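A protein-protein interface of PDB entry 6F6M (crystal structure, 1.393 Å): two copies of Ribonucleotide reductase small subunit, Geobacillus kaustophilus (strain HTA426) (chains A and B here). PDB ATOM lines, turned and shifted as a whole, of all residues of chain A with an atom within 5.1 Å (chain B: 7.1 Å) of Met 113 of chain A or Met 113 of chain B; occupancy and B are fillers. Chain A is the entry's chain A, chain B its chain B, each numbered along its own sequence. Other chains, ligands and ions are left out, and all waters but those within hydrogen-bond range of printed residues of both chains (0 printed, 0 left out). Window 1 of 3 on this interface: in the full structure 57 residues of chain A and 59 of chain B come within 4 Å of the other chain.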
ATOM      1  N   THR A  87      14.017 -20.557  -8.207  1.00  0.00           N
ATOM      2  CA  THR A  87      13.454 -20.623  -6.859  1.00  0.00           C
ATOM      3  C   THR A  87      12.879 -19.269  -6.466  1.00  0.00           C
ATOM      4  O   THR A  87      11.727 -19.162  -6.011  1.00  0.00           O
ATOM      5  CB  THR A  87      14.520 -21.061  -5.856  1.00  0.00           C
ATOM      6  OG1 THR A  87      15.001 -22.361  -6.211  1.00  0.00           O
ATOM      7  CG2 THR A  87      13.942 -21.164  -4.486  1.00  0.00           C
ATOM      8  N   LEU A  88      13.660 -18.212  -6.679  1.00  0.00           N
ATOM      9  CA  LEU A  88      13.229 -16.876  -6.302  1.00  0.00           C
ATOM     10  C   LEU A  88      12.143 -16.353  -7.233  1.00  0.00           C
ATOM     11  O   LEU A  88      11.193 -15.692  -6.785  1.00  0.00           O
ATOM     12  CB  LEU A  88      14.450 -15.951  -6.319  1.00  0.00           C
ATOM     13  CG  LEU A  88      15.642 -16.397  -5.462  1.00  0.00           C
ATOM     14  CD1 LEU A  88      16.832 -15.454  -5.569  1.00  0.00           C
ATOM     15  CD2 LEU A  88      15.263 -16.622  -3.996  1.00  0.00           C
ATOM     16  N   ILE A  90       9.834 -17.711  -9.258  1.00  0.00           N
ATOM     17  CA  ILE A  90       8.478 -18.230  -9.411  1.00  0.00           C
ATOM     18  C   ILE A  90       7.493 -17.541  -8.475  1.00  0.00           C
ATOM     19  O   ILE A  90       6.282 -17.578  -8.737  1.00  0.00           O
ATOM     20  CB  ILE A  90       8.504 -19.757  -9.225  1.00  0.00           C
ATOM     21  CG1 ILE A  90       7.179 -20.419  -9.651  1.00  0.00           C
ATOM     22  CG2 ILE A  90       8.884 -20.106  -7.818  1.00  0.00           C
ATOM     23  CD1 ILE A  90       6.867 -20.277 -11.163  1.00  0.00           C
ATOM     24  N   LEU A  91       7.972 -16.887  -7.407  1.00  0.00           N
ATOM     25  CA  LEU A  91       7.048 -16.284  -6.444  1.00  0.00           C
ATOM     26  C   LEU A  91       6.061 -15.295  -7.054  1.00  0.00           C
ATOM     27  O   LEU A  91       4.886 -15.342  -6.666  1.00  0.00           O
ATOM     28  CB  LEU A  91       7.811 -15.633  -5.286  1.00  0.00           C
ATOM     29  CG  LEU A  91       8.529 -16.615  -4.361  1.00  0.00           C
ATOM     30  CD1 LEU A  91       9.490 -15.870  -3.444  1.00  0.00           C
ATOM     31  CD2 LEU A  91       7.553 -17.415  -3.511  1.00  0.00           C
ATOM     32  N   LEU A 109       1.809 -24.922  -7.536  1.00  0.00           N
ATOM     33  CA  LEU A 109       3.036 -24.139  -7.512  1.00  0.00           C
ATOM     34  C   LEU A 109       3.785 -24.257  -6.192  1.00  0.00           C
ATOM     35  O   LEU A 109       5.007 -24.059  -6.177  1.00  0.00           O
ATOM     36  CB  LEU A 109       2.765 -22.679  -7.863  1.00  0.00           C
ATOM     37  CG  LEU A 109       2.470 -22.421  -9.334  1.00  0.00           C
ATOM     38  CD1 LEU A 109       2.136 -20.926  -9.564  1.00  0.00           C
ATOM     39  CD2 LEU A 109       3.654 -22.834 -10.220  1.00  0.00           C
ATOM     40  N   THR A 110       3.122 -24.630  -5.090  1.00  0.00           N
ATOM     41  CA  THR A 110       3.901 -24.937  -3.890  1.00  0.00           C
ATOM     42  C   THR A 110       4.857 -26.109  -4.123  1.00  0.00           C
ATOM     43  O   THR A 110       5.963 -26.115  -3.573  1.00  0.00           O
ATOM     44  CB  THR A 110       3.029 -25.206  -2.651  1.00  0.00           C
ATOM     45  OG1 THR A 110       2.338 -26.455  -2.776  1.00  0.00           O
ATOM     46  CG2 THR A 110       2.053 -24.057  -2.410  1.00  0.00           C
ATOM     47  N   THR A 111       4.450 -27.099  -4.936  1.00  0.00           N
ATOM     48  CA  THR A 111       5.343 -28.215  -5.254  1.00  0.00           C
ATOM     49  C   THR A 111       6.419 -27.782  -6.239  1.00  0.00           C
ATOM     50  O   THR A 111       7.571 -28.211  -6.129  1.00  0.00           O
ATOM     51  CB  THR A 111       4.578 -29.443  -5.777  1.00  0.00           C
ATOM     52  OG1 THR A 111       4.155 -29.284  -7.138  1.00  0.00           O
ATOM     53  CG2 THR A 111       3.373 -29.786  -4.897  1.00  0.00           C
ATOM     54  N   PHE A 112       6.067 -26.914  -7.183  1.00  0.00           N
ATOM     55  CA  PHE A 112       7.047 -26.368  -8.110  1.00  0.00           C
ATOM     56  C   PHE A 112       8.158 -25.668  -7.338  1.00  0.00           C
ATOM     57  O   PHE A 112       9.348 -25.909  -7.560  1.00  0.00           O
ATOM     58  CB  PHE A 112       6.275 -25.429  -9.037  1.00  0.00           C
ATOM     59  CG  PHE A 112       7.025 -24.907 -10.237  1.00  0.00           C
ATOM     60  CD1 PHE A 112       6.471 -25.032 -11.501  1.00  0.00           C
ATOM     61  CD2 PHE A 112       8.190 -24.173 -10.112  1.00  0.00           C
ATOM     62  CE1 PHE A 112       7.074 -24.487 -12.602  1.00  0.00           C
ATOM     63  CE2 PHE A 112       8.803 -23.628 -11.227  1.00  0.00           C
ATOM     64  CZ  PHE A 112       8.234 -23.765 -12.463  1.00  0.00           C
ATOM     65  N   MET A 113       7.785 -24.806  -6.387  1.00  0.00           N
ATOM     66  CA  MET A 113       8.800 -24.051  -5.662  1.00  0.00           C
ATOM     67  C   MET A 113       9.617 -24.948  -4.740  1.00  0.00           C
ATOM     68  O   MET A 113      10.844 -24.778  -4.621  1.00  0.00           O
ATOM     69  CB  MET A 113       8.203 -22.879  -4.909  1.00  0.00           C
ATOM     70  CG  MET A 113       9.297 -21.828  -4.654  1.00  0.00           C
ATOM     71  SD  MET A 113       8.720 -20.485  -3.645  1.00  0.00           S
ATOM     72  CE  MET A 113      10.269 -19.642  -3.274  1.00  0.00           C
ATOM     73  N   HIS A 114       8.982 -25.927  -4.104  1.00  0.00           N
ATOM     74  CA  HIS A 114       9.779 -26.819  -3.280  1.00  0.00           C
ATOM     75  C   HIS A 114      10.697 -27.696  -4.117  1.00  0.00           C
ATOM     76  O   HIS A 114      11.814 -27.979  -3.690  1.00  0.00           O
ATOM     77  CB  HIS A 114       8.911 -27.642  -2.345  1.00  0.00           C
ATOM     78  CG  HIS A 114       9.717 -28.505  -1.455  1.00  0.00           C
ATOM     79  ND1 HIS A 114      10.645 -27.994  -0.573  1.00  0.00           N
ATOM     80  CD2 HIS A 114       9.803 -29.853  -1.364  1.00  0.00           C
ATOM     81  CE1 HIS A 114      11.242 -28.996   0.050  1.00  0.00           C
ATOM     82  NE2 HIS A 114      10.724 -30.135  -0.388  1.00  0.00           N
ATOM     83  N   ASP A 115      10.273 -28.064  -5.326  1.00  0.00           N
ATOM     84  CA  ASP A 115      11.176 -28.778  -6.221  1.00  0.00           C
ATOM     85  C   ASP A 115      12.401 -27.926  -6.511  1.00  0.00           C
ATOM     86  O   ASP A 115      13.535 -28.397  -6.424  1.00  0.00           O
ATOM     87  CB  ASP A 115      10.495 -29.095  -7.547  1.00  0.00           C
ATOM     88  CG  ASP A 115       9.418 -30.160  -7.469  1.00  0.00           C
ATOM     89  OD1 ASP A 115       9.334 -30.896  -6.464  1.00  0.00           O
ATOM     90  OD2 ASP A 115       8.677 -30.232  -8.475  1.00  0.00           O
ATOM     91  N   GLU A 116      12.200 -26.637  -6.833  1.00  0.00           N
ATOM     92  CA  GLU A 116      13.358 -25.808  -7.170  1.00  0.00           C
ATOM     93  C   GLU A 116      14.307 -25.664  -5.982  1.00  0.00           C
ATOM     94  O   GLU A 116      15.536 -25.647  -6.148  1.00  0.00           O
ATOM     95  CB  GLU A 116      12.936 -24.414  -7.660  1.00  0.00           C
ATOM     96  CG  GLU A 116      11.959 -24.366  -8.826  1.00  0.00           C
ATOM     97  CD  GLU A 116      12.466 -25.017 -10.118  1.00  0.00           C
ATOM     98  OE1 GLU A 116      13.550 -25.677 -10.125  1.00  0.00           O
ATOM     99  OE2 GLU A 116      11.753 -24.898 -11.132  1.00  0.00           O
ATOM    100  N   ALA A 117      13.759 -25.539  -4.779  1.00  0.00           N
ATOM    101  CA  ALA A 117      14.585 -25.506  -3.580  1.00  0.00           C
ATOM    102  C   ALA A 117      15.494 -26.736  -3.514  1.00  0.00           C
ATOM    103  O   ALA A 117      16.697 -26.642  -3.225  1.00  0.00           O
ATOM    104  CB  ALA A 117      13.690 -25.412  -2.340  1.00  0.00           C
ATOM    105  N   VAL B  86      -3.580 -18.723   4.858  1.00  0.00           N
ATOM    106  CA  VAL B  86      -2.133 -18.760   5.081  1.00  0.00           C
ATOM    107  C   VAL B  86      -1.419 -19.288   3.853  1.00  0.00           C
ATOM    108  O   VAL B  86      -0.259 -18.924   3.605  1.00  0.00           O
ATOM    109  CB  VAL B  86      -1.710 -19.515   6.369  1.00  0.00           C
ATOM    110  CG1 VAL B  86      -2.124 -18.731   7.617  1.00  0.00           C
ATOM    111  CG2 VAL B  86      -2.267 -20.895   6.417  1.00  0.00           C
ATOM    112  N   THR B  87      -2.085 -20.145   3.065  1.00  0.00           N
ATOM    113  CA  THR B  87      -1.506 -20.589   1.800  1.00  0.00           C
ATOM    114  C   THR B  87      -1.205 -19.391   0.904  1.00  0.00           C
ATOM    115  O   THR B  87      -0.105 -19.268   0.348  1.00  0.00           O
ATOM    116  CB  THR B  87      -2.429 -21.585   1.088  1.00  0.00           C
ATOM    117  OG1 THR B  87      -2.601 -22.768   1.888  1.00  0.00           O
ATOM    118  CG2 THR B  87      -1.805 -22.006  -0.236  1.00  0.00           C
ATOM    119  N   LEU B  88      -2.174 -18.493   0.751  1.00  0.00           N
ATOM    120  CA  LEU B  88      -1.987 -17.344  -0.118  1.00  0.00           C
ATOM    121  C   LEU B  88      -1.087 -16.292   0.534  1.00  0.00           C
ATOM    122  O   LEU B  88      -0.278 -15.653  -0.149  1.00  0.00           O
ATOM    123  CB  LEU B  88      -3.353 -16.729  -0.417  1.00  0.00           C
ATOM    124  CG  LEU B  88      -4.405 -17.698  -0.957  1.00  0.00           C
ATOM    125  CD1 LEU B  88      -5.697 -16.965  -1.209  1.00  0.00           C
ATOM    126  CD2 LEU B  88      -3.937 -18.429  -2.229  1.00  0.00           C
ATOM    127  N   ILE B  90       1.355 -16.259   2.794  1.00  0.00           N
ATOM    128  CA  ILE B  90       2.786 -16.400   3.064  1.00  0.00           C
ATOM    129  C   ILE B  90       3.632 -15.912   1.900  1.00  0.00           C
ATOM    130  O   ILE B  90       4.811 -15.583   2.099  1.00  0.00           O
ATOM    131  CB  ILE B  90       3.109 -17.846   3.482  1.00  0.00           C
ATOM    132  CG1 ILE B  90       4.533 -17.978   4.012  1.00  0.00           C
ATOM    133  CG2 ILE B  90       2.890 -18.780   2.330  1.00  0.00           C
ATOM    134  CD1 ILE B  90       4.726 -17.274   5.357  1.00  0.00           C
ATOM    135  N   LEU B  91       3.050 -15.811   0.698  1.00  0.00           N
ATOM    136  CA  LEU B  91       3.837 -15.433  -0.472  1.00  0.00           C
ATOM    137  C   LEU B  91       4.549 -14.096  -0.311  1.00  0.00           C
ATOM    138  O   LEU B  91       5.716 -14.004  -0.733  1.00  0.00           O
ATOM    139  CB  LEU B  91       2.989 -15.454  -1.742  1.00  0.00           C
ATOM    140  CG  LEU B  91       2.520 -16.821  -2.212  1.00  0.00           C
ATOM    141  CD1 LEU B  91       1.482 -16.726  -3.295  1.00  0.00           C
ATOM    142  CD2 LEU B  91       3.731 -17.610  -2.704  1.00  0.00           C
ATOM    143  N   PRO B  92       3.958 -13.050   0.285  1.00  0.00           N
ATOM    144  CA  PRO B  92       4.726 -11.807   0.410  1.00  0.00           C
ATOM    145  C   PRO B  92       5.910 -11.919   1.341  1.00  0.00           C
ATOM    146  O   PRO B  92       6.903 -11.215   1.129  1.00  0.00           O
ATOM    147  CB  PRO B  92       3.693 -10.793   0.939  1.00  0.00           C
ATOM    148  CG  PRO B  92       2.373 -11.337   0.575  1.00  0.00           C
ATOM    149  CD  PRO B  92       2.544 -12.837   0.663  1.00  0.00           C
ATOM    150  N   ALA B  94       7.772 -14.661   1.708  1.00  0.00           N
ATOM    151  CA  ALA B  94       8.802 -15.320   0.920  1.00  0.00           C
ATOM    152  C   ALA B  94       9.469 -14.334  -0.019  1.00  0.00           C
ATOM    153  O   ALA B  94      10.696 -14.340  -0.172  1.00  0.00           O
ATOM    154  CB  ALA B  94       8.203 -16.496   0.125  1.00  0.00           C
ATOM    155  N   HIS B  95       8.667 -13.488  -0.674  1.00  0.00           N
ATOM    156  CA  HIS B  95       9.210 -12.465  -1.568  1.00  0.00           C
ATOM    157  C   HIS B  95      10.127 -11.509  -0.824  1.00  0.00           C
ATOM    158  O   HIS B  95      11.229 -11.202  -1.283  1.00  0.00           O
ATOM    159  CB  HIS B  95       8.083 -11.675  -2.232  1.00  0.00           C
ATOM    160  CG  HIS B  95       8.546 -10.386  -2.829  1.00  0.00           C
ATOM    161  ND1 HIS B  95       9.090 -10.310  -4.092  1.00  0.00           N
ATOM    162  CD2 HIS B  95       8.559  -9.123  -2.335  1.00  0.00           C
ATOM    163  CE1 HIS B  95       9.411  -9.057  -4.355  1.00  0.00           C
ATOM    164  NE2 HIS B  95       9.113  -8.320  -3.299  1.00  0.00           N
ATOM    165  N   ALA B  98      13.314 -13.184   0.153  1.00  0.00           N
ATOM    166  CA  ALA B  98      14.090 -13.424  -1.055  1.00  0.00           C
ATOM    167  C   ALA B  98      14.797 -12.161  -1.519  1.00  0.00           C
ATOM    168  O   ALA B  98      15.985 -12.194  -1.869  1.00  0.00           O
ATOM    169  CB  ALA B  98      13.177 -13.957  -2.153  1.00  0.00           C
ATOM    170  N   VAL B 106      14.155 -18.654   2.395  1.00  0.00           N
ATOM    171  CA  VAL B 106      13.318 -18.969   1.246  1.00  0.00           C
ATOM    172  C   VAL B 106      13.191 -20.478   1.079  1.00  0.00           C
ATOM    173  O   VAL B 106      12.102 -20.999   0.819  1.00  0.00           O
ATOM    174  CB  VAL B 106      13.857 -18.302  -0.030  1.00  0.00           C
ATOM    175  CG1 VAL B 106      13.021 -18.704  -1.245  1.00  0.00           C
ATOM    176  CG2 VAL B 106      13.844 -16.784   0.113  1.00  0.00           C
ATOM    177  N   LEU B 107      14.312 -21.201   1.161  1.00  0.00           N
ATOM    178  CA  LEU B 107      14.230 -22.659   1.020  1.00  0.00           C
ATOM    179  C   LEU B 107      13.247 -23.218   2.032  1.00  0.00           C
ATOM    180  O   LEU B 107      12.362 -24.020   1.689  1.00  0.00           O
ATOM    181  CB  LEU B 107      15.605 -23.288   1.204  1.00  0.00           C
ATOM    182  CG  LEU B 107      16.690 -22.884   0.192  1.00  0.00           C
ATOM    183  CD1 LEU B 107      18.017 -23.496   0.546  1.00  0.00           C
ATOM    184  CD2 LEU B 107      16.289 -23.217  -1.259  1.00  0.00           C
ATOM    185  N   PHE B 108      13.406 -22.827   3.300  1.00  0.00           N
ATOM    186  CA  PHE B 108      12.467 -23.278   4.322  1.00  0.00           C
ATOM    187  C   PHE B 108      11.039 -22.903   3.973  1.00  0.00           C
ATOM    188  O   PHE B 108      10.119 -23.719   4.103  1.00  0.00           O
ATOM    189  CB  PHE B 108      12.781 -22.696   5.699  1.00  0.00           C
ATOM    190  CG  PHE B 108      11.672 -22.933   6.642  1.00  0.00           C
ATOM    191  CD1 PHE B 108      11.399 -24.207   7.077  1.00  0.00           C
ATOM    192  CD2 PHE B 108      10.780 -21.904   6.962  1.00  0.00           C
ATOM    193  CE1 PHE B 108      10.289 -24.477   7.885  1.00  0.00           C
ATOM    194  CE2 PHE B 108       9.687 -22.144   7.758  1.00  0.00           C
ATOM    195  CZ  PHE B 108       9.424 -23.428   8.217  1.00  0.00           C
ATOM    196  N   LEU B 109      10.823 -21.674   3.522  1.00  0.00           N
ATOM    197  CA  LEU B 109       9.466 -21.248   3.230  1.00  0.00           C
ATOM    198  C   LEU B 109       8.814 -22.016   2.103  1.00  0.00           C
ATOM    199  O   LEU B 109       7.584 -22.090   2.086  1.00  0.00           O
ATOM    200  CB  LEU B 109       9.400 -19.729   2.988  1.00  0.00           C
ATOM    201  CG  LEU B 109       9.526 -18.897   4.275  1.00  0.00           C
ATOM    202  CD1 LEU B 109       9.569 -17.394   3.928  1.00  0.00           C
ATOM    203  CD2 LEU B 109       8.397 -19.194   5.277  1.00  0.00           C
ATOM    204  N   THR B 110       9.582 -22.640   1.209  1.00  0.00           N
ATOM    205  CA  THR B 110       8.947 -23.535   0.240  1.00  0.00           C
ATOM    206  C   THR B 110       8.273 -24.699   0.949  1.00  0.00           C
ATOM    207  O   THR B 110       7.215 -25.174   0.491  1.00  0.00           O
ATOM    208  CB  THR B 110       9.914 -24.061  -0.847  1.00  0.00           C
ATOM    209  OG1 THR B 110      10.841 -25.038  -0.322  1.00  0.00           O
ATOM    210  CG2 THR B 110      10.652 -22.927  -1.565  1.00  0.00           C
ATOM    211  N   THR B 111       8.844 -25.166   2.063  1.00  0.00           N
ATOM    212  CA  THR B 111       8.191 -26.258   2.781  1.00  0.00           C
ATOM    213  C   THR B 111       6.987 -25.745   3.563  1.00  0.00           C
ATOM    214  O   THR B 111       5.971 -26.451   3.688  1.00  0.00           O
ATOM    215  CB  THR B 111       9.157 -27.016   3.695  1.00  0.00           C
ATOM    216  OG1 THR B 111       9.482 -26.240   4.859  1.00  0.00           O
ATOM    217  CG2 THR B 111      10.414 -27.402   2.970  1.00  0.00           C
ATOM    218  N   PHE B 112       7.097 -24.517   4.098  1.00  0.00           N
ATOM    219  CA  PHE B 112       5.973 -23.873   4.767  1.00  0.00           C
ATOM    220  C   PHE B 112       4.792 -23.785   3.816  1.00  0.00           C
ATOM    221  O   PHE B 112       3.669 -24.206   4.134  1.00  0.00           O
ATOM    222  CB  PHE B 112       6.462 -22.484   5.183  1.00  0.00           C
ATOM    223  CG  PHE B 112       5.589 -21.729   6.138  1.00  0.00           C
ATOM    224  CD1 PHE B 112       6.122 -21.260   7.333  1.00  0.00           C
ATOM    225  CD2 PHE B 112       4.300 -21.370   5.811  1.00  0.00           C
ATOM    226  CE1 PHE B 112       5.361 -20.482   8.216  1.00  0.00           C
ATOM    227  CE2 PHE B 112       3.531 -20.603   6.684  1.00  0.00           C
ATOM    228  CZ  PHE B 112       4.066 -20.160   7.883  1.00  0.00           C
ATOM    229  N   MET B 113       5.038 -23.296   2.614  1.00  0.00           N
ATOM    230  CA  MET B 113       3.944 -23.121   1.671  1.00  0.00           C
ATOM    231  C   MET B 113       3.343 -24.454   1.250  1.00  0.00           C
ATOM    232  O   MET B 113       2.114 -24.597   1.154  1.00  0.00           O
ATOM    233  CB  MET B 113       4.466 -22.361   0.456  1.00  0.00           C
ATOM    234  CG  MET B 113       4.793 -20.961   0.816  1.00  0.00           C
ATOM    235  SD  MET B 113       5.106 -19.825  -0.510  1.00  0.00           S
ATOM    236  CE  MET B 113       6.552 -20.562  -1.050  1.00  0.00           C
ATOM    237  N   HIS B 114       4.192 -25.445   0.987  1.00  0.00           N
ATOM    238  CA  HIS B 114       3.641 -26.722   0.565  1.00  0.00           C
ATOM    239  C   HIS B 114       2.907 -27.408   1.711  1.00  0.00           C
ATOM    240  O   HIS B 114       1.913 -28.115   1.476  1.00  0.00           O
ATOM    241  CB  HIS B 114       4.695 -27.623  -0.034  1.00  0.00           C
ATOM    242  CG  HIS B 114       4.126 -28.925  -0.482  1.00  0.00           C
ATOM    243  ND1 HIS B 114       3.095 -29.007  -1.397  1.00  0.00           N
ATOM    244  CD2 HIS B 114       4.403 -30.194  -0.101  1.00  0.00           C
ATOM    245  CE1 HIS B 114       2.773 -30.282  -1.567  1.00  0.00           C
ATOM    246  NE2 HIS B 114       3.571 -31.024  -0.816  1.00  0.00           N
ATOM    247  N   ASP B 115       3.367 -27.210   2.959  1.00  0.00           N
ATOM    248  CA  ASP B 115       2.590 -27.652   4.118  1.00  0.00           C
ATOM    249  C   ASP B 115       1.194 -27.046   4.089  1.00  0.00           C
ATOM    250  O   ASP B 115       0.195 -27.741   4.249  1.00  0.00           O
ATOM    251  CB  ASP B 115       3.269 -27.262   5.432  1.00  0.00           C
ATOM    252  CG  ASP B 115       4.540 -28.031   5.735  1.00  0.00           C
ATOM    253  OD1 ASP B 115       4.835 -29.084   5.116  1.00  0.00           O
ATOM    254  OD2 ASP B 115       5.244 -27.590   6.671  1.00  0.00           O
ATOM    255  N   GLU B 116       1.099 -25.727   3.899  1.00  0.00           N
ATOM    256  CA  GLU B 116      -0.223 -25.104   3.948  1.00  0.00           C
ATOM    257  C   GLU B 116      -1.129 -25.631   2.851  1.00  0.00           C
ATOM    258  O   GLU B 116      -2.341 -25.776   3.054  1.00  0.00           O
ATOM    259  CB  GLU B 116      -0.115 -23.582   3.857  1.00  0.00           C
ATOM    260  CG  GLU B 116       0.748 -22.876   4.926  1.00  0.00           C
ATOM    261  CD  GLU B 116       0.331 -23.127   6.346  1.00  0.00           C
ATOM    262  OE1 GLU B 116      -0.555 -23.969   6.609  1.00  0.00           O
ATOM    263  OE2 GLU B 116       0.881 -22.436   7.220  1.00  0.00           O
ATOM    264  N   ALA B 117      -0.574 -25.893   1.669  1.00  0.00           N
ATOM    265  CA  ALA B 117      -1.362 -26.517   0.602  1.00  0.00           C
ATOM    266  C   ALA B 117      -1.968 -27.827   1.082  1.00  0.00           C
ATOM    267  O   ALA B 117      -3.147 -28.116   0.832  1.00  0.00           O
ATOM    268  CB  ALA B 117      -0.488 -26.761  -0.634  1.00  0.00           C
ATOM    269  N   LYS B 118      -1.162 -28.656   1.729  1.00  0.00           N
ATOM    270  CA  LYS B 118      -1.693 -29.910   2.254  1.00  0.00           C
ATOM    271  C   LYS B 118      -2.767 -29.667   3.299  1.00  0.00           C
ATOM    272  O   LYS B 118      -3.741 -30.421   3.360  1.00  0.00           O
ATOM    273  CB  LYS B 118      -0.575 -30.779   2.832  1.00  0.00           C
ATOM    274  CG  LYS B 118       0.441 -31.158   1.775  1.00  0.00           C
ATOM    275  CD  LYS B 118       1.332 -32.289   2.164  1.00  0.00           C
ATOM    276  CE  LYS B 118       2.352 -31.929   3.173  1.00  0.00           C
ATOM    277  NZ  LYS B 118       3.382 -33.048   3.356  1.00  0.00           N
ATOM    278  N   HIS B 119      -2.631 -28.598   4.103  1.00  0.00           N
ATOM    279  CA  HIS B 119      -3.623 -28.344   5.145  1.00  0.00           C
ATOM    280  C   HIS B 119      -4.963 -27.917   4.554  1.00  0.00           C
ATOM    281  O   HIS B 119      -6.023 -28.407   4.988  1.00  0.00           O
ATOM    282  CB  HIS B 119      -3.101 -27.259   6.091  1.00  0.00           C
ATOM    283  CG  HIS B 119      -1.837 -27.638   6.778  1.00  0.00           C
ATOM    284  ND1 HIS B 119      -1.143 -26.785   7.625  1.00  0.00           N
ATOM    285  CD2 HIS B 119      -1.131 -28.791   6.721  1.00  0.00           C
ATOM    286  CE1 HIS B 119      -0.050 -27.422   8.037  1.00  0.00           C
ATOM    287  NE2 HIS B 119      -0.022 -28.636   7.491  1.00  0.00           N
ATOM    288  N   HIS B 219       6.359 -23.986  11.592  1.00  0.00           N
ATOM    289  CA  HIS B 219       5.924 -22.671  11.145  1.00  0.00           C
ATOM    290  C   HIS B 219       6.074 -21.662  12.268  1.00  0.00           C
ATOM    291  O   HIS B 219       6.549 -20.540  12.054  1.00  0.00           O
ATOM    292  CB  HIS B 219       4.471 -22.741  10.655  1.00  0.00           C
ATOM    293  CG  HIS B 219       4.268 -23.693   9.515  1.00  0.00           C
ATOM    294  ND1 HIS B 219       3.101 -23.747   8.783  1.00  0.00           N
ATOM    295  CD2 HIS B 219       5.080 -24.649   9.001  1.00  0.00           C
ATOM    296  CE1 HIS B 219       3.213 -24.690   7.863  1.00  0.00           C
ATOM    297  NE2 HIS B 219       4.410 -25.223   7.954  1.00  0.00           N
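The side-chain hydroxyl (OG1) of Thr 110 of chain B lies within hydrogen-bond range of a ring nitrogen (ND1) of His 114 of chain A (3.0 Å).
A ring nitrogen (ND1) of His 114 of chain B lies within hydrogen-bond range of the side-chain hydroxyl of Thr 110 of chain A (3.0 Å).
The side-chain hydroxyl (OG1) of Thr 110 of chain B is in hydrogen-bond range of the backbone carbonyl oxygen (O) of Leu 107 of chain B.
The backbone carbonyl oxygen of Phe 108 of chain B sits at hydrogen-bond distance from the side-chain hydroxyl of Thr 111 of chain B (2.7 Å).
CD2 of Leu 88 of chain A touches CB of Ala 98 of chain B (3.9 Å).
Leu 91 of chain A touches Ala 94 of chain B.
CD1 of Leu 91 of chain A touches N of His 95 of chain B, 3.7 Å away.
Met 113 of chain B touches Thr 110 of chain A.
Thr 111 of chain A touches His 114 of chain B (CG2 to CE1, 3.4 Å).
Val 106 of chain B touches Met 113 of chain A (CG1 to CE, 3.5 Å).
CG2 of Thr 110 of chain B touches CG of Met 113 of chain A, 3.5 Å away.
Met 113 of chain A touches Met 113 of chain B.
His 114 of chain A touches Thr 111 of chain B (CE1 to CG2, 3.4 Å).
Ala 117 of chain A touches Thr 110 of chain B.
Printed residues of chain B within 4 Å of Met 113 of chain A: Val 106, Thr 110 and Met 113.
Of the printed residues of chain A, Met 113 of chain B touches Thr 110 and Met 113.
Printed residues of chain B within 4 Å of Thr 111 of chain A: His 114.
Of the printed residues of chain A, Leu 107 of chain B touches Ala 117 (3.6 Å).
Of the printed residues of chain B, His 114 of chain A touches Thr 110 and Thr 111.
Thr 87 of chain B touches none of the printed residues of chain A.
Glu 116 of chain A touches none of the printed residues of chain B.
The nearest printed residue of chain B that does not touch Met 113 of chain A is Ala 94 of chain B (5.1 Å).
The nearest printed residue of chain A that does not touch Met 113 of chain B is Leu 91 of chain A (4.1 Å).
The nearest printed residue of chain B that does not touch His 114 of chain A is His 114 of chain B (4.8 Å).
Of the 24 printed residues of chain B, 11 touch a printed residue of chain A.
Printed residues of chain B that touch a printed residue of chain A: Leu 91, Ala 94, His 95, Ala 98, Val 106, Leu 107, Thr 110, Thr 111, Met 113, His 114 and Ala 117.
Hydrophobic or aromatic side chains of chain B within 4 Å of the printed part of chain A: Leu 91, Ala 94, Ala 98, Val 106, Leu 107, Met 113, His 114 and Ala 117.
Along chain B the printed residues that touch a printed residue of chain A span positions 91 to 117.
Hydrophobic or aromatic side chains of chain A within 4 Å of the printed part of chain B: Leu 88, Leu 91, Met 113, His 114 and Ala 117.
Along chain A the printed residues that touch a printed residue of chain B span positions 88 to 117.
Leu 91 of chain A touches its own counterpart, Leu 91 of chain B.
Thr 110 of chain A touches Met 113 of chain B, and with the chains exchanged Met 113 of chain A touches Thr 110 of chain B.
Thr 110 of chain A touches His 114 of chain B, and with the chains exchanged His 114 of chain A touches Thr 110 of chain B.
Thr 110 of chain A touches Ala 117 of chain B, and with the chains exchanged Ala 117 of chain A touches Thr 110 of chain B.
13 positions are printed for both chains.
Of the 15 pairs that touch across the chains among the printed residues, 10 have their exchanged pair printed and touching as well.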
